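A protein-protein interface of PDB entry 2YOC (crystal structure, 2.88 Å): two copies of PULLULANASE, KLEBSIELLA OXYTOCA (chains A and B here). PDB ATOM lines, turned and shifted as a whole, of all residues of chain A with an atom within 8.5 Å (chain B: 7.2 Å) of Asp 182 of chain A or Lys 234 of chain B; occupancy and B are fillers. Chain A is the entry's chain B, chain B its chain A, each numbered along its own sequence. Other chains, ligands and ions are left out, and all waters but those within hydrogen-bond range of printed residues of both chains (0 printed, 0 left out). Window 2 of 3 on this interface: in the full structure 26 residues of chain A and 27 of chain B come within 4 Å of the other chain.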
ATOM      1  N   TRP A 177     -36.597  20.635 -24.505  1.00  0.00           N
ATOM      2  CA  TRP A 177     -35.501  19.823 -25.025  1.00  0.00           C
ATOM      3  C   TRP A 177     -34.130  20.418 -24.718  1.00  0.00           C
ATOM      4  O   TRP A 177     -33.750  21.435 -25.314  1.00  0.00           O
ATOM      5  CB  TRP A 177     -35.665  19.551 -26.528  1.00  0.00           C
ATOM      6  CG  TRP A 177     -34.665  18.586 -27.100  1.00  0.00           C
ATOM      7  CD1 TRP A 177     -34.066  17.536 -26.460  1.00  0.00           C
ATOM      8  CD2 TRP A 177     -34.240  18.518 -28.467  1.00  0.00           C
ATOM      9  NE1 TRP A 177     -33.260  16.847 -27.333  1.00  0.00           N
ATOM     10  CE2 TRP A 177     -33.347  17.429 -28.576  1.00  0.00           C
ATOM     11  CE3 TRP A 177     -34.472  19.317 -29.604  1.00  0.00           C
ATOM     12  CZ2 TRP A 177     -32.699  17.110 -29.780  1.00  0.00           C
ATOM     13  CZ3 TRP A 177     -33.837  18.994 -30.792  1.00  0.00           C
ATOM     14  CH2 TRP A 177     -32.979  17.892 -30.878  1.00  0.00           C
ATOM     15  N   PRO A 178     -33.352  19.770 -23.827  1.00  0.00           N
ATOM     16  CA  PRO A 178     -31.986  20.271 -23.559  1.00  0.00           C
ATOM     17  C   PRO A 178     -31.042  20.166 -24.791  1.00  0.00           C
ATOM     18  O   PRO A 178     -30.138  20.996 -24.956  1.00  0.00           O
ATOM     19  CB  PRO A 178     -31.498  19.410 -22.380  1.00  0.00           C
ATOM     20  CG  PRO A 178     -32.657  18.575 -21.972  1.00  0.00           C
ATOM     21  CD  PRO A 178     -33.645  18.538 -23.071  1.00  0.00           C
ATOM     22  N   GLY A 179     -31.284  19.168 -25.645  1.00  0.00           N
ATOM     23  CA  GLY A 179     -30.489  18.939 -26.842  1.00  0.00           C
ATOM     24  C   GLY A 179     -30.526  20.052 -27.871  1.00  0.00           C
ATOM     25  O   GLY A 179     -29.593  20.204 -28.655  1.00  0.00           O
ATOM     26  N   GLY A 180     -31.610  20.805 -27.889  1.00  0.00           N
ATOM     27  CA  GLY A 180     -31.797  21.900 -28.827  1.00  0.00           C
ATOM     28  C   GLY A 180     -31.369  23.238 -28.275  1.00  0.00           C
ATOM     29  O   GLY A 180     -31.560  24.264 -28.937  1.00  0.00           O
ATOM     30  N   GLN A 181     -30.810  23.248 -27.050  1.00  0.00           N
ATOM     31  CA  GLN A 181     -30.345  24.462 -26.365  1.00  0.00           C
ATOM     32  C   GLN A 181     -29.176  25.101 -27.130  1.00  0.00           C
ATOM     33  O   GLN A 181     -28.198  24.408 -27.457  1.00  0.00           O
ATOM     34  CB  GLN A 181     -29.939  24.147 -24.906  1.00  0.00           C
ATOM     35  CG  GLN A 181     -29.180  25.251 -24.193  1.00  0.00           C
ATOM     36  CD  GLN A 181     -29.944  25.763 -23.014  1.00  0.00           C
ATOM     37  OE1 GLN A 181     -29.811  25.264 -21.866  1.00  0.00           O
ATOM     38  NE2 GLN A 181     -30.744  26.794 -23.271  1.00  0.00           N
ATOM     39  N   ASP A 182     -29.303  26.423 -27.411  1.00  0.00           N
ATOM     40  CA  ASP A 182     -28.332  27.266 -28.109  1.00  0.00           C
ATOM     41  C   ASP A 182     -28.078  26.883 -29.579  1.00  0.00           C
ATOM     42  O   ASP A 182     -27.254  27.526 -30.242  1.00  0.00           O
ATOM     43  CB  ASP A 182     -27.019  27.396 -27.310  1.00  0.00           C
ATOM     44  CG  ASP A 182     -27.135  27.953 -25.881  1.00  0.00           C
ATOM     45  OD1 ASP A 182     -27.912  28.919 -25.677  1.00  0.00           O
ATOM     46  OD2 ASP A 182     -26.378  27.471 -24.983  1.00  0.00           O
ATOM     47  N   LYS A 183     -28.797  25.868 -30.109  1.00  0.00           N
ATOM     48  CA  LYS A 183     -28.623  25.416 -31.495  1.00  0.00           C
ATOM     49  C   LYS A 183     -29.280  26.386 -32.480  1.00  0.00           C
ATOM     50  O   LYS A 183     -30.346  26.924 -32.153  1.00  0.00           O
ATOM     51  CB  LYS A 183     -29.098  23.968 -31.679  1.00  0.00           C
ATOM     52  CG  LYS A 183     -28.506  22.982 -30.665  1.00  0.00           C
ATOM     53  CD  LYS A 183     -26.982  22.982 -30.673  1.00  0.00           C
ATOM     54  CE  LYS A 183     -26.367  21.977 -29.741  1.00  0.00           C
ATOM     55  NZ  LYS A 183     -26.746  20.579 -30.078  1.00  0.00           N
ATOM     56  N   PRO A 184     -28.614  26.693 -33.637  1.00  0.00           N
ATOM     57  CA  PRO A 184     -29.184  27.675 -34.596  1.00  0.00           C
ATOM     58  C   PRO A 184     -30.512  27.249 -35.248  1.00  0.00           C
ATOM     59  O   PRO A 184     -31.436  28.070 -35.355  1.00  0.00           O
ATOM     60  CB  PRO A 184     -28.055  27.884 -35.618  1.00  0.00           C
ATOM     61  CG  PRO A 184     -27.225  26.683 -35.534  1.00  0.00           C
ATOM     62  CD  PRO A 184     -27.327  26.152 -34.132  1.00  0.00           C
ATOM     63  N   ILE A 185     -30.621  25.960 -35.638  1.00  0.00           N
ATOM     64  CA  ILE A 185     -31.850  25.401 -36.199  1.00  0.00           C
ATOM     65  C   ILE A 185     -32.509  24.418 -35.192  1.00  0.00           C
ATOM     66  O   ILE A 185     -31.890  23.417 -34.802  1.00  0.00           O
ATOM     67  CB  ILE A 185     -31.636  24.780 -37.618  1.00  0.00           C
ATOM     68  CG1 ILE A 185     -31.237  25.838 -38.684  1.00  0.00           C
ATOM     69  CG2 ILE A 185     -32.856  23.962 -38.055  1.00  0.00           C
ATOM     70  CD1 ILE A 185     -32.304  27.021 -38.949  1.00  0.00           C
ATOM     71  N   VAL A 186     -33.756  24.742 -34.760  1.00  0.00           N
ATOM     72  CA  VAL A 186     -34.558  23.902 -33.850  1.00  0.00           C
ATOM     73  C   VAL A 186     -35.936  23.745 -34.472  1.00  0.00           C
ATOM     74  O   VAL A 186     -36.655  24.735 -34.664  1.00  0.00           O
ATOM     75  CB  VAL A 186     -34.587  24.385 -32.359  1.00  0.00           C
ATOM     76  CG1 VAL A 186     -35.578  23.576 -31.533  1.00  0.00           C
ATOM     77  CG2 VAL A 186     -33.200  24.308 -31.724  1.00  0.00           C
ATOM     78  N   PRO A 213     -36.677  29.935 -29.167  1.00  0.00           N
ATOM     79  CA  PRO A 213     -36.377  29.849 -27.729  1.00  0.00           C
ATOM     80  C   PRO A 213     -37.312  30.687 -26.860  1.00  0.00           C
ATOM     81  O   PRO A 213     -37.623  31.839 -27.183  1.00  0.00           O
ATOM     82  CB  PRO A 213     -34.927  30.320 -27.644  1.00  0.00           C
ATOM     83  CG  PRO A 213     -34.712  31.129 -28.878  1.00  0.00           C
ATOM     84  CD  PRO A 213     -35.527  30.469 -29.921  1.00  0.00           C
ATOM     85  N   SER A 229     -35.603  22.745 -15.556  1.00  0.00           N
ATOM     86  CA  SER A 229     -34.271  23.162 -15.990  1.00  0.00           C
ATOM     87  C   SER A 229     -34.076  22.991 -17.508  1.00  0.00           C
ATOM     88  O   SER A 229     -33.201  23.640 -18.081  1.00  0.00           O
ATOM     89  CB  SER A 229     -33.198  22.397 -15.217  1.00  0.00           C
ATOM     90  OG  SER A 229     -33.085  21.030 -15.596  1.00  0.00           O
ATOM     91  N   ALA A 231     -34.416  23.191 -21.621  1.00  0.00           N
ATOM     92  CA  ALA A 231     -34.523  24.281 -22.588  1.00  0.00           C
ATOM     93  C   ALA A 231     -35.920  24.336 -23.214  1.00  0.00           C
ATOM     94  O   ALA A 231     -36.352  23.359 -23.851  1.00  0.00           O
ATOM     95  CB  ALA A 231     -33.467  24.116 -23.675  1.00  0.00           C
ATOM     96  N   ALA A 232     -36.618  25.486 -23.038  1.00  0.00           N
ATOM     97  CA  ALA A 232     -37.974  25.714 -23.564  1.00  0.00           C
ATOM     98  C   ALA A 232     -37.996  26.298 -24.978  1.00  0.00           C
ATOM     99  O   ALA A 232     -37.201  27.187 -25.289  1.00  0.00           O
ATOM    100  CB  ALA A 232     -38.775  26.605 -22.616  1.00  0.00           C
ATOM    101  N   PHE A 233     -38.926  25.791 -25.822  1.00  0.00           N
ATOM    102  CA  PHE A 233     -39.143  26.244 -27.201  1.00  0.00           C
ATOM    103  C   PHE A 233     -40.621  26.467 -27.490  1.00  0.00           C
ATOM    104  O   PHE A 233     -41.442  25.590 -27.209  1.00  0.00           O
ATOM    105  CB  PHE A 233     -38.558  25.256 -28.227  1.00  0.00           C
ATOM    106  CG  PHE A 233     -37.090  24.990 -28.024  1.00  0.00           C
ATOM    107  CD1 PHE A 233     -36.661  23.969 -27.187  1.00  0.00           C
ATOM    108  CD2 PHE A 233     -36.129  25.777 -28.649  1.00  0.00           C
ATOM    109  CE1 PHE A 233     -35.296  23.729 -26.995  1.00  0.00           C
ATOM    110  CE2 PHE A 233     -34.772  25.529 -28.453  1.00  0.00           C
ATOM    111  CZ  PHE A 233     -34.369  24.513 -27.620  1.00  0.00           C
ATOM    112  N   ALA A 253     -32.400  19.306 -34.244  1.00  0.00           N
ATOM    113  CA  ALA A 253     -31.395  20.345 -34.024  1.00  0.00           C
ATOM    114  C   ALA A 253     -30.337  20.252 -35.146  1.00  0.00           C
ATOM    115  O   ALA A 253     -29.766  19.177 -35.411  1.00  0.00           O
ATOM    116  CB  ALA A 253     -30.757  20.211 -32.641  1.00  0.00           C
ATOM    117  N   ALA A 254     -30.131  21.386 -35.839  1.00  0.00           N
ATOM    118  CA  ALA A 254     -29.195  21.496 -36.948  1.00  0.00           C
ATOM    119  C   ALA A 254     -28.349  22.762 -36.889  1.00  0.00           C
ATOM    120  O   ALA A 254     -28.707  23.753 -36.225  1.00  0.00           O
ATOM    121  CB  ALA A 254     -29.942  21.428 -38.270  1.00  0.00           C
ATOM    122  N   ILE A 261     -27.462  17.846 -36.113  1.00  0.00           N
ATOM    123  CA  ILE A 261     -26.683  17.675 -34.897  1.00  0.00           C
ATOM    124  C   ILE A 261     -27.367  16.513 -34.178  1.00  0.00           C
ATOM    125  O   ILE A 261     -26.746  15.466 -33.954  1.00  0.00           O
ATOM    126  CB  ILE A 261     -26.596  18.978 -34.029  1.00  0.00           C
ATOM    127  CG1 ILE A 261     -26.278  20.239 -34.874  1.00  0.00           C
ATOM    128  CG2 ILE A 261     -25.580  18.811 -32.892  1.00  0.00           C
ATOM    129  CD1 ILE A 261     -26.435  21.582 -34.145  1.00  0.00           C
ATOM    130  N   ASN B 173     -19.793  30.385 -21.066  1.00  0.00           N
ATOM    131  CA  ASN B 173     -21.102  29.796 -20.758  1.00  0.00           C
ATOM    132  C   ASN B 173     -21.145  28.314 -20.318  1.00  0.00           C
ATOM    133  O   ASN B 173     -22.136  27.892 -19.732  1.00  0.00           O
ATOM    134  CB  ASN B 173     -21.972  29.963 -21.993  1.00  0.00           C
ATOM    135  CG  ASN B 173     -23.394  30.343 -21.706  1.00  0.00           C
ATOM    136  OD1 ASN B 173     -23.717  31.060 -20.730  1.00  0.00           O
ATOM    137  ND2 ASN B 173     -24.277  29.922 -22.605  1.00  0.00           N
ATOM    138  N   THR B 174     -20.116  27.523 -20.637  1.00  0.00           N
ATOM    139  CA  THR B 174     -20.133  26.079 -20.424  1.00  0.00           C
ATOM    140  C   THR B 174     -19.246  25.499 -19.333  1.00  0.00           C
ATOM    141  O   THR B 174     -18.051  25.809 -19.256  1.00  0.00           O
ATOM    142  CB  THR B 174     -19.976  25.402 -21.782  1.00  0.00           C
ATOM    143  OG1 THR B 174     -20.955  25.959 -22.658  1.00  0.00           O
ATOM    144  CG2 THR B 174     -20.147  23.897 -21.723  1.00  0.00           C
ATOM    145  N   LEU B 175     -19.835  24.604 -18.530  1.00  0.00           N
ATOM    146  CA  LEU B 175     -19.147  23.884 -17.468  1.00  0.00           C
ATOM    147  C   LEU B 175     -19.391  22.401 -17.715  1.00  0.00           C
ATOM    148  O   LEU B 175     -20.557  21.970 -17.769  1.00  0.00           O
ATOM    149  CB  LEU B 175     -19.651  24.358 -16.085  1.00  0.00           C
ATOM    150  CG  LEU B 175     -19.139  23.713 -14.775  1.00  0.00           C
ATOM    151  CD1 LEU B 175     -19.869  22.448 -14.431  1.00  0.00           C
ATOM    152  CD2 LEU B 175     -17.655  23.560 -14.727  1.00  0.00           C
ATOM    153  N   VAL B 186     -27.636  21.220  -9.594  1.00  0.00           N
ATOM    154  CA  VAL B 186     -26.293  21.419 -10.166  1.00  0.00           C
ATOM    155  C   VAL B 186     -25.965  22.905 -10.065  1.00  0.00           C
ATOM    156  O   VAL B 186     -26.669  23.743 -10.658  1.00  0.00           O
ATOM    157  CB  VAL B 186     -26.094  20.832 -11.595  1.00  0.00           C
ATOM    158  CG1 VAL B 186     -24.757  21.243 -12.184  1.00  0.00           C
ATOM    159  CG2 VAL B 186     -26.197  19.313 -11.576  1.00  0.00           C
ATOM    160  N   LEU B 209     -24.324  29.921  -8.518  1.00  0.00           N
ATOM    161  CA  LEU B 209     -25.039  30.139  -9.772  1.00  0.00           C
ATOM    162  C   LEU B 209     -25.742  28.832 -10.123  1.00  0.00           C
ATOM    163  O   LEU B 209     -25.176  27.759  -9.904  1.00  0.00           O
ATOM    164  CB  LEU B 209     -24.126  30.519 -10.950  1.00  0.00           C
ATOM    165  CG  LEU B 209     -23.093  31.643 -10.840  1.00  0.00           C
ATOM    166  CD1 LEU B 209     -22.299  31.711 -12.116  1.00  0.00           C
ATOM    167  CD2 LEU B 209     -23.731  32.975 -10.579  1.00  0.00           C
ATOM    168  N   LYS B 210     -26.962  28.906 -10.675  1.00  0.00           N
ATOM    169  CA  LYS B 210     -27.701  27.695 -11.035  1.00  0.00           C
ATOM    170  C   LYS B 210     -27.322  27.227 -12.419  1.00  0.00           C
ATOM    171  O   LYS B 210     -27.302  28.014 -13.374  1.00  0.00           O
ATOM    172  CB  LYS B 210     -29.215  27.851 -10.821  1.00  0.00           C
ATOM    173  CG  LYS B 210     -29.560  27.665  -9.325  1.00  0.00           C
ATOM    174  CD  LYS B 210     -31.062  27.590  -8.951  1.00  0.00           C
ATOM    175  CE  LYS B 210     -31.632  26.181  -8.959  1.00  0.00           C
ATOM    176  NZ  LYS B 210     -31.644  25.536  -7.618  1.00  0.00           N
ATOM    177  N   LEU B 211     -26.942  25.963 -12.523  1.00  0.00           N
ATOM    178  CA  LEU B 211     -26.543  25.420 -13.828  1.00  0.00           C
ATOM    179  C   LEU B 211     -27.683  24.606 -14.444  1.00  0.00           C
ATOM    180  O   LEU B 211     -28.440  23.956 -13.726  1.00  0.00           O
ATOM    181  CB  LEU B 211     -25.224  24.614 -13.741  1.00  0.00           C
ATOM    182  CG  LEU B 211     -24.015  25.334 -13.132  1.00  0.00           C
ATOM    183  CD1 LEU B 211     -22.884  24.388 -12.896  1.00  0.00           C
ATOM    184  CD2 LEU B 211     -23.554  26.454 -14.016  1.00  0.00           C
ATOM    185  N   THR B 212     -27.840  24.686 -15.767  1.00  0.00           N
ATOM    186  CA  THR B 212     -28.934  24.024 -16.488  1.00  0.00           C
ATOM    187  C   THR B 212     -28.348  23.077 -17.510  1.00  0.00           C
ATOM    188  O   THR B 212     -27.381  23.461 -18.179  1.00  0.00           O
ATOM    189  CB  THR B 212     -29.854  25.052 -17.169  1.00  0.00           C
ATOM    190  OG1 THR B 212     -29.257  25.478 -18.401  1.00  0.00           O
ATOM    191  CG2 THR B 212     -30.181  26.258 -16.276  1.00  0.00           C
ATOM    192  N   PRO B 213     -28.913  21.860 -17.685  1.00  0.00           N
ATOM    193  CA  PRO B 213     -28.353  20.932 -18.669  1.00  0.00           C
ATOM    194  C   PRO B 213     -28.379  21.461 -20.105  1.00  0.00           C
ATOM    195  O   PRO B 213     -29.380  22.051 -20.549  1.00  0.00           O
ATOM    196  CB  PRO B 213     -29.208  19.681 -18.492  1.00  0.00           C
ATOM    197  CG  PRO B 213     -30.451  20.149 -17.869  1.00  0.00           C
ATOM    198  CD  PRO B 213     -30.059  21.258 -16.985  1.00  0.00           C
ATOM    199  N   THR B 214     -27.235  21.315 -20.791  1.00  0.00           N
ATOM    200  CA  THR B 214     -27.040  21.708 -22.191  1.00  0.00           C
ATOM    201  C   THR B 214     -26.220  20.669 -22.945  1.00  0.00           C
ATOM    202  O   THR B 214     -25.857  19.628 -22.401  1.00  0.00           O
ATOM    203  CB  THR B 214     -26.523  23.174 -22.329  1.00  0.00           C
ATOM    204  OG1 THR B 214     -26.675  23.597 -23.683  1.00  0.00           O
ATOM    205  CG2 THR B 214     -25.071  23.344 -21.917  1.00  0.00           C
ATOM    206  N   THR B 215     -25.935  20.944 -24.189  1.00  0.00           N
ATOM    207  CA  THR B 215     -25.140  20.039 -24.993  1.00  0.00           C
ATOM    208  C   THR B 215     -23.794  20.689 -25.354  1.00  0.00           C
ATOM    209  O   THR B 215     -23.707  21.917 -25.563  1.00  0.00           O
ATOM    210  CB  THR B 215     -25.948  19.525 -26.197  1.00  0.00           C
ATOM    211  OG1 THR B 215     -26.678  20.610 -26.802  1.00  0.00           O
ATOM    212  CG2 THR B 215     -26.890  18.407 -25.807  1.00  0.00           C
ATOM    213  N   ALA B 232     -22.624  18.439 -20.158  1.00  0.00           N
ATOM    214  CA  ALA B 232     -22.576  19.898 -20.324  1.00  0.00           C
ATOM    215  C   ALA B 232     -23.644  20.640 -19.537  1.00  0.00           C
ATOM    216  O   ALA B 232     -24.797  20.173 -19.465  1.00  0.00           O
ATOM    217  CB  ALA B 232     -22.657  20.270 -21.798  1.00  0.00           C
ATOM    218  N   PHE B 233     -23.257  21.804 -18.947  1.00  0.00           N
ATOM    219  CA  PHE B 233     -24.140  22.687 -18.157  1.00  0.00           C
ATOM    220  C   PHE B 233     -23.964  24.136 -18.545  1.00  0.00           C
ATOM    221  O   PHE B 233     -22.836  24.621 -18.617  1.00  0.00           O
ATOM    222  CB  PHE B 233     -23.922  22.535 -16.650  1.00  0.00           C
ATOM    223  CG  PHE B 233     -24.085  21.112 -16.163  1.00  0.00           C
ATOM    224  CD1 PHE B 233     -23.001  20.229 -16.154  1.00  0.00           C
ATOM    225  CD2 PHE B 233     -25.328  20.638 -15.758  1.00  0.00           C
ATOM    226  CE1 PHE B 233     -23.159  18.918 -15.727  1.00  0.00           C
ATOM    227  CE2 PHE B 233     -25.480  19.322 -15.329  1.00  0.00           C
ATOM    228  CZ  PHE B 233     -24.394  18.476 -15.319  1.00  0.00           C
ATOM    229  N   LYS B 234     -25.091  24.828 -18.803  1.00  0.00           N
ATOM    230  CA  LYS B 234     -25.150  26.237 -19.188  1.00  0.00           C
ATOM    231  C   LYS B 234     -25.151  27.089 -17.930  1.00  0.00           C
ATOM    232  O   LYS B 234     -25.887  26.786 -16.993  1.00  0.00           O
ATOM    233  CB  LYS B 234     -26.413  26.506 -20.028  1.00  0.00           C
ATOM    234  CG  LYS B 234     -26.390  27.808 -20.811  1.00  0.00           C
ATOM    235  CD  LYS B 234     -27.755  28.159 -21.402  1.00  0.00           C
ATOM    236  CE  LYS B 234     -27.712  29.216 -22.491  1.00  0.00           C
ATOM    237  NZ  LYS B 234     -27.460  30.581 -21.989  1.00  0.00           N
ATOM    238  N   LEU B 235     -24.293  28.119 -17.885  1.00  0.00           N
ATOM    239  CA  LEU B 235     -24.194  29.050 -16.755  1.00  0.00           C
ATOM    240  C   LEU B 235     -25.273  30.105 -16.946  1.00  0.00           C
ATOM    241  O   LEU B 235     -25.623  30.366 -18.116  1.00  0.00           O
ATOM    242  CB  LEU B 235     -22.818  29.749 -16.755  1.00  0.00           C
ATOM    243  CG  LEU B 235     -21.741  29.185 -15.844  1.00  0.00           C
ATOM    244  CD1 LEU B 235     -20.974  28.079 -16.529  1.00  0.00           C
ATOM    245  CD2 LEU B 235     -20.768  30.269 -15.425  1.00  0.00           C
ATOM    246  N   PRO B 236     -25.771  30.792 -15.871  1.00  0.00           N
ATOM    247  CA  PRO B 236     -26.767  31.863 -16.085  1.00  0.00           C
ATOM    248  C   PRO B 236     -26.243  33.000 -16.972  1.00  0.00           C
ATOM    249  O   PRO B 236     -25.031  33.128 -17.156  1.00  0.00           O
ATOM    250  CB  PRO B 236     -27.076  32.344 -14.666  1.00  0.00           C
ATOM    251  CG  PRO B 236     -25.964  31.919 -13.838  1.00  0.00           C
ATOM    252  CD  PRO B 236     -25.459  30.643 -14.433  1.00  0.00           C
ATOM    253  N   ASP B 237     -27.138  33.791 -17.558  1.00  0.00           N
ATOM    254  CA  ASP B 237     -26.716  34.897 -18.410  1.00  0.00           C
ATOM    255  C   ASP B 237     -26.176  36.085 -17.608  1.00  0.00           C
ATOM    256  O   ASP B 237     -25.331  36.830 -18.096  1.00  0.00           O
ATOM    257  CB  ASP B 237     -27.830  35.284 -19.394  1.00  0.00           C
ATOM    258  CG  ASP B 237     -28.119  34.193 -20.426  1.00  0.00           C
ATOM    259  OD1 ASP B 237     -27.149  33.560 -20.917  1.00  0.00           O
ATOM    260  OD2 ASP B 237     -29.313  33.964 -20.733  1.00  0.00           O
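Of the 18 printed residues of chain A, 6 touch a printed residue of chain B.
Hydrophobic or aromatic side chains of chain A within 4 Å of the printed part of chain B: Pro 178.
Along chain B the printed residues that touch a printed residue of chain A span positions 212 to 234.
Among the printed residues, 11 pairs touch across the chains.
Positions printed for both chains: 186, 213, 232 and 233.
The backbone carbonyl oxygen (O) of Thr 212 of chain B sits at hydrogen-bond distance from the backbone NH (N) of Lys 234 of chain B, at 2.7 Å.
The side-chain amino group (NZ) of Lys 234 of chain B lies close to the side-chain amide nitrogen (ND2) of Asn 173 of chain B.
The side-chain carboxylate (OD1) of Asp 237 of chain B lies within salt-bridge range of the side-chain amino group (NZ) of Lys 234 of chain B.
The backbone NH (N) of Thr 214 of chain B lies within hydrogen-bond range of the backbone carbonyl oxygen (O) of Ala 232 of chain B (3.0 Å).
The backbone carbonyl oxygen of Gly 179 of chain A sits at hydrogen-bond distance from the side-chain amino group of Lys 183 of chain A (3.2 Å).
O of Gly 179 of chain A is in hydrogen-bond range of OG1 of Thr 215 of chain B (3.5 Å).
OG1 of Thr 215 of chain B lies close to NZ of Lys 183 of chain A (3.3 Å).
The side-chain amide oxygen of Gln 181 of chain A lies close to the backbone carbonyl oxygen of Pro 213 of chain B.
Of the printed residues of chain B, Asp 182 of chain A touches Lys 234 (3.2 Å).
Of the printed residues of chain A, Thr 212 of chain B touches Gln 181 (3.5 Å) and Ser 229 (3.7 Å).
Of the printed residues of chain A, Pro 213 of chain B touches Pro 178 (3.8 Å), Gln 181 (3.5 Å) and Ser 229 (3.3 Å).
Of the printed residues of chain A, Thr 215 of chain B touches Pro 178 (3.9 Å), Gly 179 (3.5 Å) and Lys 183 (3.3 Å).
Lys 234 of chain B touches just these residues of chain A: Gln 181 and Asp 182.
The nearest printed residue of chain B that does not touch Asp 182 of chain A is Asn 173 of chain B (4.01 Å).
The nearest residue of chain A that does not touch Lys 234 of chain B is Ala 231 of chain A (7.4 Å).
Pro 178 of chain A touches Pro 213 of chain B.
Pro 178 of chain A touches Thr 215 of chain B (O to OG1, 3.9 Å).
Gln 181 of chain A touches Thr 212 of chain B (OE1 to OG1, 3.5 Å).
Thr 214 of chain B touches Gln 181 of chain A.
Gln 181 of chain A touches Lys 234 of chain B.
Lys 234 of chain B touches Asp 182 of chain A.
Ser 229 of chain A touches Thr 212 of chain B (O to CB, 3.7 Å).
Ser 229 of chain A touches Pro 213 of chain B (OG to CD, 3.3 Å).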
